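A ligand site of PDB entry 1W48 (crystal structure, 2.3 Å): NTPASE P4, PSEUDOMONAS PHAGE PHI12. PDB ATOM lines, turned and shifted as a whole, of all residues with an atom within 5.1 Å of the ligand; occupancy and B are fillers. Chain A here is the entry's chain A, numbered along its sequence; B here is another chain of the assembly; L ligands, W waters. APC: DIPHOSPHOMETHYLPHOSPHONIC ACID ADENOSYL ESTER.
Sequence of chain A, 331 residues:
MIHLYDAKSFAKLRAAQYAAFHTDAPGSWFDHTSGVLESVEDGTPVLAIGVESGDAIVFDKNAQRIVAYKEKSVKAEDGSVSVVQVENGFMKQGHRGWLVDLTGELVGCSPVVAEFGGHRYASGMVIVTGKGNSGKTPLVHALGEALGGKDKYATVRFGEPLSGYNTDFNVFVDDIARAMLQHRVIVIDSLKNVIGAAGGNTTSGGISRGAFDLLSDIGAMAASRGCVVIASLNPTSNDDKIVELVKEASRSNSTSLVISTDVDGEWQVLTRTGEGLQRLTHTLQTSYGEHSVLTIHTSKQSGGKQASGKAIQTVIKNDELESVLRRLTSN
N of Thr 137 is in hydrogen-bond range of O2A of the ligand (2.8 Å).
The backbone NH of Lys 136 is in hydrogen-bond range of an oxygen (O1A) of the ligand, 3.0 Å away.
OG of Ser 252 of chain B sits at hydrogen-bond distance from O1G of the ligand (3.2 Å).
An oxygen (O2G) of the ligand sits close to the side-chain carboxylate (OE1) of Glu 160, at 2.8 Å.
O2A of the ligand is in hydrogen-bond range of OG1 of Thr 137, at 3.1 Å.
The side-chain hydroxyl of Ser 292 lies within hydrogen-bond range of a nitrogen (N7) of the ligand.
The side-chain amide oxygen of Asn 234 sits close to an oxygen (O3G) of the ligand, at 2.5 Å.
A nitrogen (N9) of the ligand sits close to the side-chain hydroxyl (OH) of Tyr 288 (3.5 Å).
Asn 133 touches the ligand (O to O3', 3.6 Å).
CA of Gly 135 touches C4' of the ligand, 3.2 Å away.
CG of Pro 138 touches O4' of the ligand, at 3.8 Å.
O of Arg 251 of chain B touches O1G of the ligand, 3.7 Å away.
NH2 of Arg 272 of chain B touches O3B of the ligand (3.8 Å).
Gly 276 of chain B touches the ligand.
Leu 277 of chain B touches the ligand (O to C2', 3.8 Å).
Gln 278 of chain B touches the ligand (CG to C5, 3.4 Å).
Lys 310 of chain B touches the ligand.
Hydrophobic or aromatic side chains within 4 Å of the ligand: Pro 138 and Tyr 288.
The nearest printed residue that does not touch the ligand is Arg 279 of chain B (4.1 Å).
Water W1 lies within hydrogen-bond range of O3' of the ligand (2.7 Å), N of Lys 310 of chain B (2.9 Å) and O of Asn 133 (3.1 Å).
Water W2 lies within hydrogen-bond range of the backbone carbonyl oxygen (O) of Ser 308 of chain B (2.5 Å), an oxygen (O2') of the ligand (2.9 Å), the backbone NH (N) of Arg 279 of chain B (2.9 Å) and the side-chain amino group (NZ) of Lys 310 of chain B (3.0 Å).
Water W4 lies within hydrogen-bond range of O2B of the ligand (3.0 Å), NZ of Lys 310 of chain B (3.0 Å), O of Leu 277 of chain B (3.3 Å) and NH1 of Arg 279 of chain B (3.4 Å).
Water W3 lies within hydrogen-bond range of O of Gly 289 (2.8 Å), N of Ser 292 (3.1 Å) and N6 of the ligand (3.1 Å).
Water W5 bridges NE of Arg 272 of chain B (2.8 Å) and O2B of the ligand (3.3 Å).
OD1 of Asn 133 sits at hydrogen-bond distance from N of Lys 310 of chain B.
O of Arg 251 of chain B lies within hydrogen-bond range of NH2 of Arg 279 of chain B.
The guanidinium group (NH2) of Arg 272 of chain B lies within salt-bridge range of the side-chain carboxylate (OE2) of Glu 160.
OE1 of Glu 160 is in hydrogen-bond range of OG of Ser 190, 2.8 Å away.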
ATOM      1  N   ASN A 133     -11.020  15.879 -15.440  1.00  0.00           N
ATOM      2  CA  ASN A 133     -11.561  14.520 -15.446  1.00  0.00           C
ATOM      3  C   ASN A 133     -10.744  13.431 -14.777  1.00  0.00           C
ATOM      4  O   ASN A 133     -11.237  12.313 -14.623  1.00  0.00           O
ATOM      5  CB  ASN A 133     -11.873  14.085 -16.883  1.00  0.00           C
ATOM      6  CG  ASN A 133     -13.002  14.890 -17.497  1.00  0.00           C
ATOM      7  OD1 ASN A 133     -13.925  15.317 -16.799  1.00  0.00           O
ATOM      8  ND2 ASN A 133     -12.951  15.079 -18.807  1.00  0.00           N
ATOM      9  N   SER A 134      -9.517  13.730 -14.374  1.00  0.00           N
ATOM     10  CA  SER A 134      -8.719  12.693 -13.728  1.00  0.00           C
ATOM     11  C   SER A 134      -9.280  12.412 -12.333  1.00  0.00           C
ATOM     12  O   SER A 134      -9.393  13.322 -11.514  1.00  0.00           O
ATOM     13  CB  SER A 134      -7.248  13.113 -13.652  1.00  0.00           C
ATOM     14  OG  SER A 134      -6.702  13.229 -14.965  1.00  0.00           O
ATOM     15  N   GLY A 135      -9.639  11.158 -12.092  1.00  0.00           N
ATOM     16  CA  GLY A 135     -10.206  10.780 -10.805  1.00  0.00           C
ATOM     17  C   GLY A 135      -9.239  10.763  -9.635  1.00  0.00           C
ATOM     18  O   GLY A 135      -8.148  10.219  -9.732  1.00  0.00           O
ATOM     19  N   LYS A 136      -9.659  11.344  -8.516  1.00  0.00           N
ATOM     20  CA  LYS A 136      -8.838  11.403  -7.318  1.00  0.00           C
ATOM     21  C   LYS A 136      -8.741  10.072  -6.551  1.00  0.00           C
ATOM     22  O   LYS A 136      -7.653   9.640  -6.188  1.00  0.00           O
ATOM     23  CB  LYS A 136      -9.382  12.468  -6.368  1.00  0.00           C
ATOM     24  CG  LYS A 136      -9.046  13.903  -6.710  1.00  0.00           C
ATOM     25  CD  LYS A 136      -9.657  14.346  -8.012  1.00  0.00           C
ATOM     26  CE  LYS A 136      -9.863  15.853  -8.019  1.00  0.00           C
ATOM     27  NZ  LYS A 136     -10.342  16.321  -9.331  1.00  0.00           N
ATOM     28  N   THR A 137      -9.890   9.434  -6.305  1.00  0.00           N
ATOM     29  CA  THR A 137      -9.903   8.189  -5.556  1.00  0.00           C
ATOM     30  C   THR A 137      -8.997   7.106  -6.139  1.00  0.00           C
ATOM     31  O   THR A 137      -8.199   6.523  -5.410  1.00  0.00           O
ATOM     32  CB  THR A 137     -11.359   7.657  -5.383  1.00  0.00           C
ATOM     33  OG1 THR A 137     -12.063   8.527  -4.487  1.00  0.00           O
ATOM     34  CG2 THR A 137     -11.381   6.275  -4.802  1.00  0.00           C
ATOM     35  N   PRO A 138      -9.106   6.830  -7.455  1.00  0.00           N
ATOM     36  CA  PRO A 138      -8.250   5.804  -8.052  1.00  0.00           C
ATOM     37  C   PRO A 138      -6.771   6.125  -7.843  1.00  0.00           C
ATOM     38  O   PRO A 138      -5.957   5.215  -7.632  1.00  0.00           O
ATOM     39  CB  PRO A 138      -8.650   5.835  -9.529  1.00  0.00           C
ATOM     40  CG  PRO A 138     -10.105   6.215  -9.462  1.00  0.00           C
ATOM     41  CD  PRO A 138     -10.096   7.317  -8.429  1.00  0.00           C
ATOM     42  N   GLU A 160     -18.673   9.772   2.455  1.00  0.00           N
ATOM     43  CA  GLU A 160     -19.087   9.501   1.078  1.00  0.00           C
ATOM     44  C   GLU A 160     -20.375   8.689   1.248  1.00  0.00           C
ATOM     45  O   GLU A 160     -20.463   7.838   2.133  1.00  0.00           O
ATOM     46  CB  GLU A 160     -18.027   8.673   0.323  1.00  0.00           C
ATOM     47  CG  GLU A 160     -16.745   9.436   0.034  1.00  0.00           C
ATOM     48  CD  GLU A 160     -16.954  10.571  -0.958  1.00  0.00           C
ATOM     49  OE1 GLU A 160     -16.089  11.462  -1.051  1.00  0.00           O
ATOM     50  OE2 GLU A 160     -17.984  10.579  -1.648  1.00  0.00           O
ATOM     51  N   SER A 190     -11.700  10.806   1.613  1.00  0.00           N
ATOM     52  CA  SER A 190     -12.420  12.028   1.762  1.00  0.00           C
ATOM     53  C   SER A 190     -12.198  13.015   2.898  1.00  0.00           C
ATOM     54  O   SER A 190     -12.720  12.880   3.999  1.00  0.00           O
ATOM     55  CB  SER A 190     -13.898  11.843   1.512  1.00  0.00           C
ATOM     56  OG  SER A 190     -14.256  12.820   0.537  1.00  0.00           O
ATOM     57  N   LYS A 192     -13.142  15.822   2.276  1.00  0.00           N
ATOM     58  CA  LYS A 192     -14.267  16.674   1.889  1.00  0.00           C
ATOM     59  C   LYS A 192     -15.122  17.226   3.028  1.00  0.00           C
ATOM     60  O   LYS A 192     -15.277  18.439   3.164  1.00  0.00           O
ATOM     61  CB  LYS A 192     -15.177  15.929   0.916  1.00  0.00           C
ATOM     62  CG  LYS A 192     -15.489  16.721  -0.340  1.00  0.00           C
ATOM     63  CD  LYS A 192     -16.782  16.259  -1.015  1.00  0.00           C
ATOM     64  CE  LYS A 192     -17.950  16.392  -0.042  1.00  0.00           C
ATOM     65  NZ  LYS A 192     -17.795  17.657   0.726  1.00  0.00           N
ATOM     66  N   ASN A 234     -11.403  16.817  -3.255  1.00  0.00           N
ATOM     67  CA  ASN A 234     -12.096  17.253  -4.449  1.00  0.00           C
ATOM     68  C   ASN A 234     -12.603  18.674  -4.271  1.00  0.00           C
ATOM     69  O   ASN A 234     -13.521  18.923  -3.485  1.00  0.00           O
ATOM     70  CB  ASN A 234     -13.270  16.309  -4.726  1.00  0.00           C
ATOM     71  CG  ASN A 234     -13.411  16.000  -6.201  1.00  0.00           C
ATOM     72  OD1 ASN A 234     -13.733  14.879  -6.587  1.00  0.00           O
ATOM     73  ND2 ASN A 234     -13.181  16.991  -7.035  1.00  0.00           N
ATOM     74  N   THR A 236     -14.782  20.770  -5.220  1.00  0.00           N
ATOM     75  CA  THR A 236     -16.069  20.892  -5.888  1.00  0.00           C
ATOM     76  C   THR A 236     -16.687  22.289  -5.884  1.00  0.00           C
ATOM     77  O   THR A 236     -16.885  22.877  -6.942  1.00  0.00           O
ATOM     78  CB  THR A 236     -17.109  19.907  -5.286  1.00  0.00           C
ATOM     79  OG1 THR A 236     -17.250  20.153  -3.889  1.00  0.00           O
ATOM     80  CG2 THR A 236     -16.667  18.469  -5.510  1.00  0.00           C
ATOM     81  N   TYR A 288      -5.858   3.217 -16.500  1.00  0.00           N
ATOM     82  CA  TYR A 288      -6.792   2.294 -15.872  1.00  0.00           C
ATOM     83  C   TYR A 288      -6.693   0.893 -16.453  1.00  0.00           C
ATOM     84  O   TYR A 288      -6.339   0.703 -17.609  1.00  0.00           O
ATOM     85  CB  TYR A 288      -8.231   2.808 -16.073  1.00  0.00           C
ATOM     86  CG  TYR A 288      -8.572   4.032 -15.264  1.00  0.00           C
ATOM     87  CD1 TYR A 288      -8.873   3.929 -13.888  1.00  0.00           C
ATOM     88  CD2 TYR A 288      -8.578   5.293 -15.844  1.00  0.00           C
ATOM     89  CE1 TYR A 288      -9.175   5.051 -13.140  1.00  0.00           C
ATOM     90  CE2 TYR A 288      -8.880   6.433 -15.089  1.00  0.00           C
ATOM     91  CZ  TYR A 288      -9.178   6.297 -13.737  1.00  0.00           C
ATOM     92  OH  TYR A 288      -9.480   7.406 -12.984  1.00  0.00           O
ATOM     93  N   GLY A 289      -7.024  -0.082 -15.623  1.00  0.00           N
ATOM     94  CA  GLY A 289      -7.037  -1.482 -16.018  1.00  0.00           C
ATOM     95  C   GLY A 289      -8.419  -1.965 -15.610  1.00  0.00           C
ATOM     96  O   GLY A 289      -9.351  -1.165 -15.552  1.00  0.00           O
ATOM     97  N   SER A 292     -11.478  -0.248 -12.917  1.00  0.00           N
ATOM     98  CA  SER A 292     -10.956   1.058 -12.552  1.00  0.00           C
ATOM     99  C   SER A 292      -9.719   1.060 -11.642  1.00  0.00           C
ATOM    100  O   SER A 292      -9.480   2.028 -10.926  1.00  0.00           O
ATOM    101  CB  SER A 292     -12.074   1.873 -11.907  1.00  0.00           C
ATOM    102  OG  SER A 292     -13.197   1.926 -12.773  1.00  0.00           O
ATOM    103  N   ARG B 251     -24.289  16.881  -5.589  1.00  0.00           N
ATOM    104  CA  ARG B 251     -23.059  16.319  -6.116  1.00  0.00           C
ATOM    105  C   ARG B 251     -22.341  15.312  -5.215  1.00  0.00           C
ATOM    106  O   ARG B 251     -21.932  14.251  -5.676  1.00  0.00           O
ATOM    107  CB  ARG B 251     -22.073  17.450  -6.455  1.00  0.00           C
ATOM    108  CG  ARG B 251     -20.774  16.941  -7.072  1.00  0.00           C
ATOM    109  CD  ARG B 251     -19.657  17.962  -7.019  1.00  0.00           C
ATOM    110  NE  ARG B 251     -19.915  19.134  -7.847  1.00  0.00           N
ATOM    111  CZ  ARG B 251     -20.326  20.316  -7.391  1.00  0.00           C
ATOM    112  NH1 ARG B 251     -20.535  20.503  -6.101  1.00  0.00           N
ATOM    113  NH2 ARG B 251     -20.507  21.308  -8.244  1.00  0.00           N
ATOM    114  N   SER B 252     -22.240  15.621  -3.930  1.00  0.00           N
ATOM    115  CA  SER B 252     -21.477  14.782  -3.007  1.00  0.00           C
ATOM    116  C   SER B 252     -22.147  14.005  -1.877  1.00  0.00           C
ATOM    117  O   SER B 252     -21.567  13.045  -1.373  1.00  0.00           O
ATOM    118  CB  SER B 252     -20.366  15.643  -2.412  1.00  0.00           C
ATOM    119  OG  SER B 252     -19.652  16.288  -3.452  1.00  0.00           O
ATOM    120  N   ARG B 272     -23.996   6.852  -9.138  1.00  0.00           N
ATOM    121  CA  ARG B 272     -22.649   6.533  -8.689  1.00  0.00           C
ATOM    122  C   ARG B 272     -22.684   5.034  -8.508  1.00  0.00           C
ATOM    123  O   ARG B 272     -23.596   4.506  -7.886  1.00  0.00           O
ATOM    124  CB  ARG B 272     -22.309   7.251  -7.382  1.00  0.00           C
ATOM    125  CG  ARG B 272     -22.179   8.753  -7.607  1.00  0.00           C
ATOM    126  CD  ARG B 272     -21.853   9.539  -6.359  1.00  0.00           C
ATOM    127  NE  ARG B 272     -20.605   9.114  -5.725  1.00  0.00           N
ATOM    128  CZ  ARG B 272     -20.074   9.720  -4.664  1.00  0.00           C
ATOM    129  NH1 ARG B 272     -20.681  10.772  -4.139  1.00  0.00           N
ATOM    130  NH2 ARG B 272     -18.955   9.272  -4.129  1.00  0.00           N
ATOM    131  N   GLY B 276     -15.028   5.965  -6.239  1.00  0.00           N
ATOM    132  CA  GLY B 276     -14.098   6.220  -7.324  1.00  0.00           C
ATOM    133  C   GLY B 276     -14.407   5.519  -8.643  1.00  0.00           C
ATOM    134  O   GLY B 276     -13.534   5.429  -9.508  1.00  0.00           O
ATOM    135  N   LEU B 277     -15.614   4.995  -8.812  1.00  0.00           N
ATOM    136  CA  LEU B 277     -15.972   4.338 -10.063  1.00  0.00           C
ATOM    137  C   LEU B 277     -16.601   5.409 -10.972  1.00  0.00           C
ATOM    138  O   LEU B 277     -16.827   6.538 -10.540  1.00  0.00           O
ATOM    139  CB  LEU B 277     -16.949   3.188  -9.808  1.00  0.00           C
ATOM    140  CG  LEU B 277     -16.276   1.804  -9.680  1.00  0.00           C
ATOM    141  CD1 LEU B 277     -14.961   1.942  -8.955  1.00  0.00           C
ATOM    142  CD2 LEU B 277     -17.196   0.819  -8.979  1.00  0.00           C
ATOM    143  N   GLN B 278     -16.867   5.073 -12.220  1.00  0.00           N
ATOM    144  CA  GLN B 278     -17.468   6.075 -13.089  1.00  0.00           C
ATOM    145  C   GLN B 278     -18.969   6.176 -12.828  1.00  0.00           C
ATOM    146  O   GLN B 278     -19.616   5.212 -12.417  1.00  0.00           O
ATOM    147  CB  GLN B 278     -17.255   5.713 -14.561  1.00  0.00           C
ATOM    148  CG  GLN B 278     -15.817   5.548 -14.965  1.00  0.00           C
ATOM    149  CD  GLN B 278     -15.672   4.818 -16.294  1.00  0.00           C
ATOM    150  OE1 GLN B 278     -15.499   5.431 -17.348  1.00  0.00           O
ATOM    151  NE2 GLN B 278     -15.757   3.489 -16.242  1.00  0.00           N
ATOM    152  N   ARG B 279     -19.505   7.362 -13.058  1.00  0.00           N
ATOM    153  CA  ARG B 279     -20.928   7.596 -12.896  1.00  0.00           C
ATOM    154  C   ARG B 279     -21.671   7.165 -14.178  1.00  0.00           C
ATOM    155  O   ARG B 279     -21.168   7.339 -15.296  1.00  0.00           O
ATOM    156  CB  ARG B 279     -21.184   9.076 -12.635  1.00  0.00           C
ATOM    157  CG  ARG B 279     -20.903   9.538 -11.191  1.00  0.00           C
ATOM    158  CD  ARG B 279     -21.304  10.988 -11.066  1.00  0.00           C
ATOM    159  NE  ARG B 279     -21.801  11.397  -9.756  1.00  0.00           N
ATOM    160  CZ  ARG B 279     -21.048  11.898  -8.770  1.00  0.00           C
ATOM    161  NH1 ARG B 279     -19.754  12.060  -8.942  1.00  0.00           N
ATOM    162  NH2 ARG B 279     -21.606  12.266  -7.636  1.00  0.00           N
ATOM    163  N   SER B 308     -20.325   8.708 -17.827  1.00  0.00           N
ATOM    164  CA  SER B 308     -20.166  10.149 -18.031  1.00  0.00           C
ATOM    165  C   SER B 308     -18.938  10.641 -17.230  1.00  0.00           C
ATOM    166  O   SER B 308     -18.676  10.138 -16.130  1.00  0.00           O
ATOM    167  CB  SER B 308     -21.440  10.911 -17.599  1.00  0.00           C
ATOM    168  OG  SER B 308     -21.568  10.969 -16.192  1.00  0.00           O
ATOM    169  N   GLY B 309     -18.196  11.593 -17.778  1.00  0.00           N
ATOM    170  CA  GLY B 309     -17.016  12.121 -17.098  1.00  0.00           C
ATOM    171  C   GLY B 309     -17.316  13.363 -16.299  1.00  0.00           C
ATOM    172  O   GLY B 309     -18.429  13.883 -16.356  1.00  0.00           O
ATOM    173  N   LYS B 310     -16.336  13.853 -15.535  1.00  0.00           N
ATOM    174  CA  LYS B 310     -16.545  15.052 -14.723  1.00  0.00           C
ATOM    175  C   LYS B 310     -17.018  16.267 -15.534  1.00  0.00           C
ATOM    176  O   LYS B 310     -17.777  17.091 -15.034  1.00  0.00           O
ATOM    177  CB  LYS B 310     -15.271  15.418 -13.950  1.00  0.00           C
ATOM    178  CG  LYS B 310     -15.318  15.070 -12.466  1.00  0.00           C
ATOM    179  CD  LYS B 310     -15.586  13.584 -12.172  1.00  0.00           C
ATOM    180  CE  LYS B 310     -17.076  13.229 -12.276  1.00  0.00           C
ATOM    181  NZ  LYS B 310     -17.378  11.817 -11.878  1.00  0.00           N
HETATM  182  PG  APC L   1     -16.859  13.210  -5.002  1.00  0.00           P
HETATM  183  O1G APC L   1     -18.299  13.923  -5.054  1.00  0.00           O
HETATM  184  O2G APC L   1     -16.707  12.596  -3.523  1.00  0.00           O
HETATM  185  O3G APC L   1     -15.759  14.148  -5.323  1.00  0.00           O
HETATM  186  PB  APC L   1     -15.656  10.992  -6.198  1.00  0.00           P
HETATM  187  O1B APC L   1     -15.164  10.626  -4.842  1.00  0.00           O
HETATM  188  O2B APC L   1     -16.019   9.900  -7.132  1.00  0.00           O
HETATM  189  O3B APC L   1     -16.938  11.952  -6.010  1.00  0.00           O
HETATM  190  PA  APC L   1     -13.237  11.158  -7.889  1.00  0.00           P
HETATM  191  O1A APC L   1     -12.536  12.099  -8.783  1.00  0.00           O
HETATM  192  O2A APC L   1     -12.441  10.377  -6.917  1.00  0.00           O
HETATM  193  C3A APC L   1     -14.460  12.111  -6.967  1.00  0.00           C
HETATM  194  O5' APC L   1     -14.175  10.165  -8.741  1.00  0.00           O
HETATM  195  C5' APC L   1     -13.644   9.056  -9.482  1.00  0.00           C
HETATM  196  C4' APC L   1     -13.159   9.499 -10.859  1.00  0.00           C
HETATM  197  O4' APC L   1     -12.518   8.373 -11.488  1.00  0.00           O
HETATM  198  C3' APC L   1     -14.314   9.919 -11.780  1.00  0.00           C
HETATM  199  O3' APC L   1     -13.906  11.008 -12.609  1.00  0.00           O
HETATM  200  C2' APC L   1     -14.501   8.665 -12.633  1.00  0.00           C
HETATM  201  O2' APC L   1     -15.053   9.045 -13.903  1.00  0.00           O
HETATM  202  C1' APC L   1     -13.031   8.286 -12.830  1.00  0.00           C
HETATM  203  N9  APC L   1     -12.886   6.894 -13.294  1.00  0.00           N
HETATM  204  C8  APC L   1     -13.083   5.812 -12.550  1.00  0.00           C
HETATM  205  N7  APC L   1     -12.847   4.713 -13.262  1.00  0.00           N
HETATM  206  C5  APC L   1     -12.489   5.093 -14.482  1.00  0.00           C
HETATM  207  C6  APC L   1     -12.152   4.401 -15.634  1.00  0.00           C
HETATM  208  N6  APC L   1     -12.132   3.075 -15.625  1.00  0.00           N
HETATM  209  N1  APC L   1     -11.849   5.124 -16.803  1.00  0.00           N
HETATM  210  C2  APC L   1     -11.887   6.525 -16.760  1.00  0.00           C
HETATM  211  N3  APC L   1     -12.208   7.153 -15.634  1.00  0.00           N
HETATM  212  C4  APC L   1     -12.509   6.494 -14.515  1.00  0.00           C
HETATM  213  O   HOH W   1     -14.238  11.874 -15.144  1.00  0.00           O
HETATM  214  O   HOH W   2     -17.873   9.657 -13.842  1.00  0.00           O
HETATM  215  O   HOH W   3     -11.922  -0.014 -15.937  1.00  0.00           O
HETATM  216  O   HOH W   4     -17.496   9.693  -9.734  1.00  0.00           O
HETATM  217  O   HOH W   5     -18.377   7.619  -6.610  1.00  0.00           O
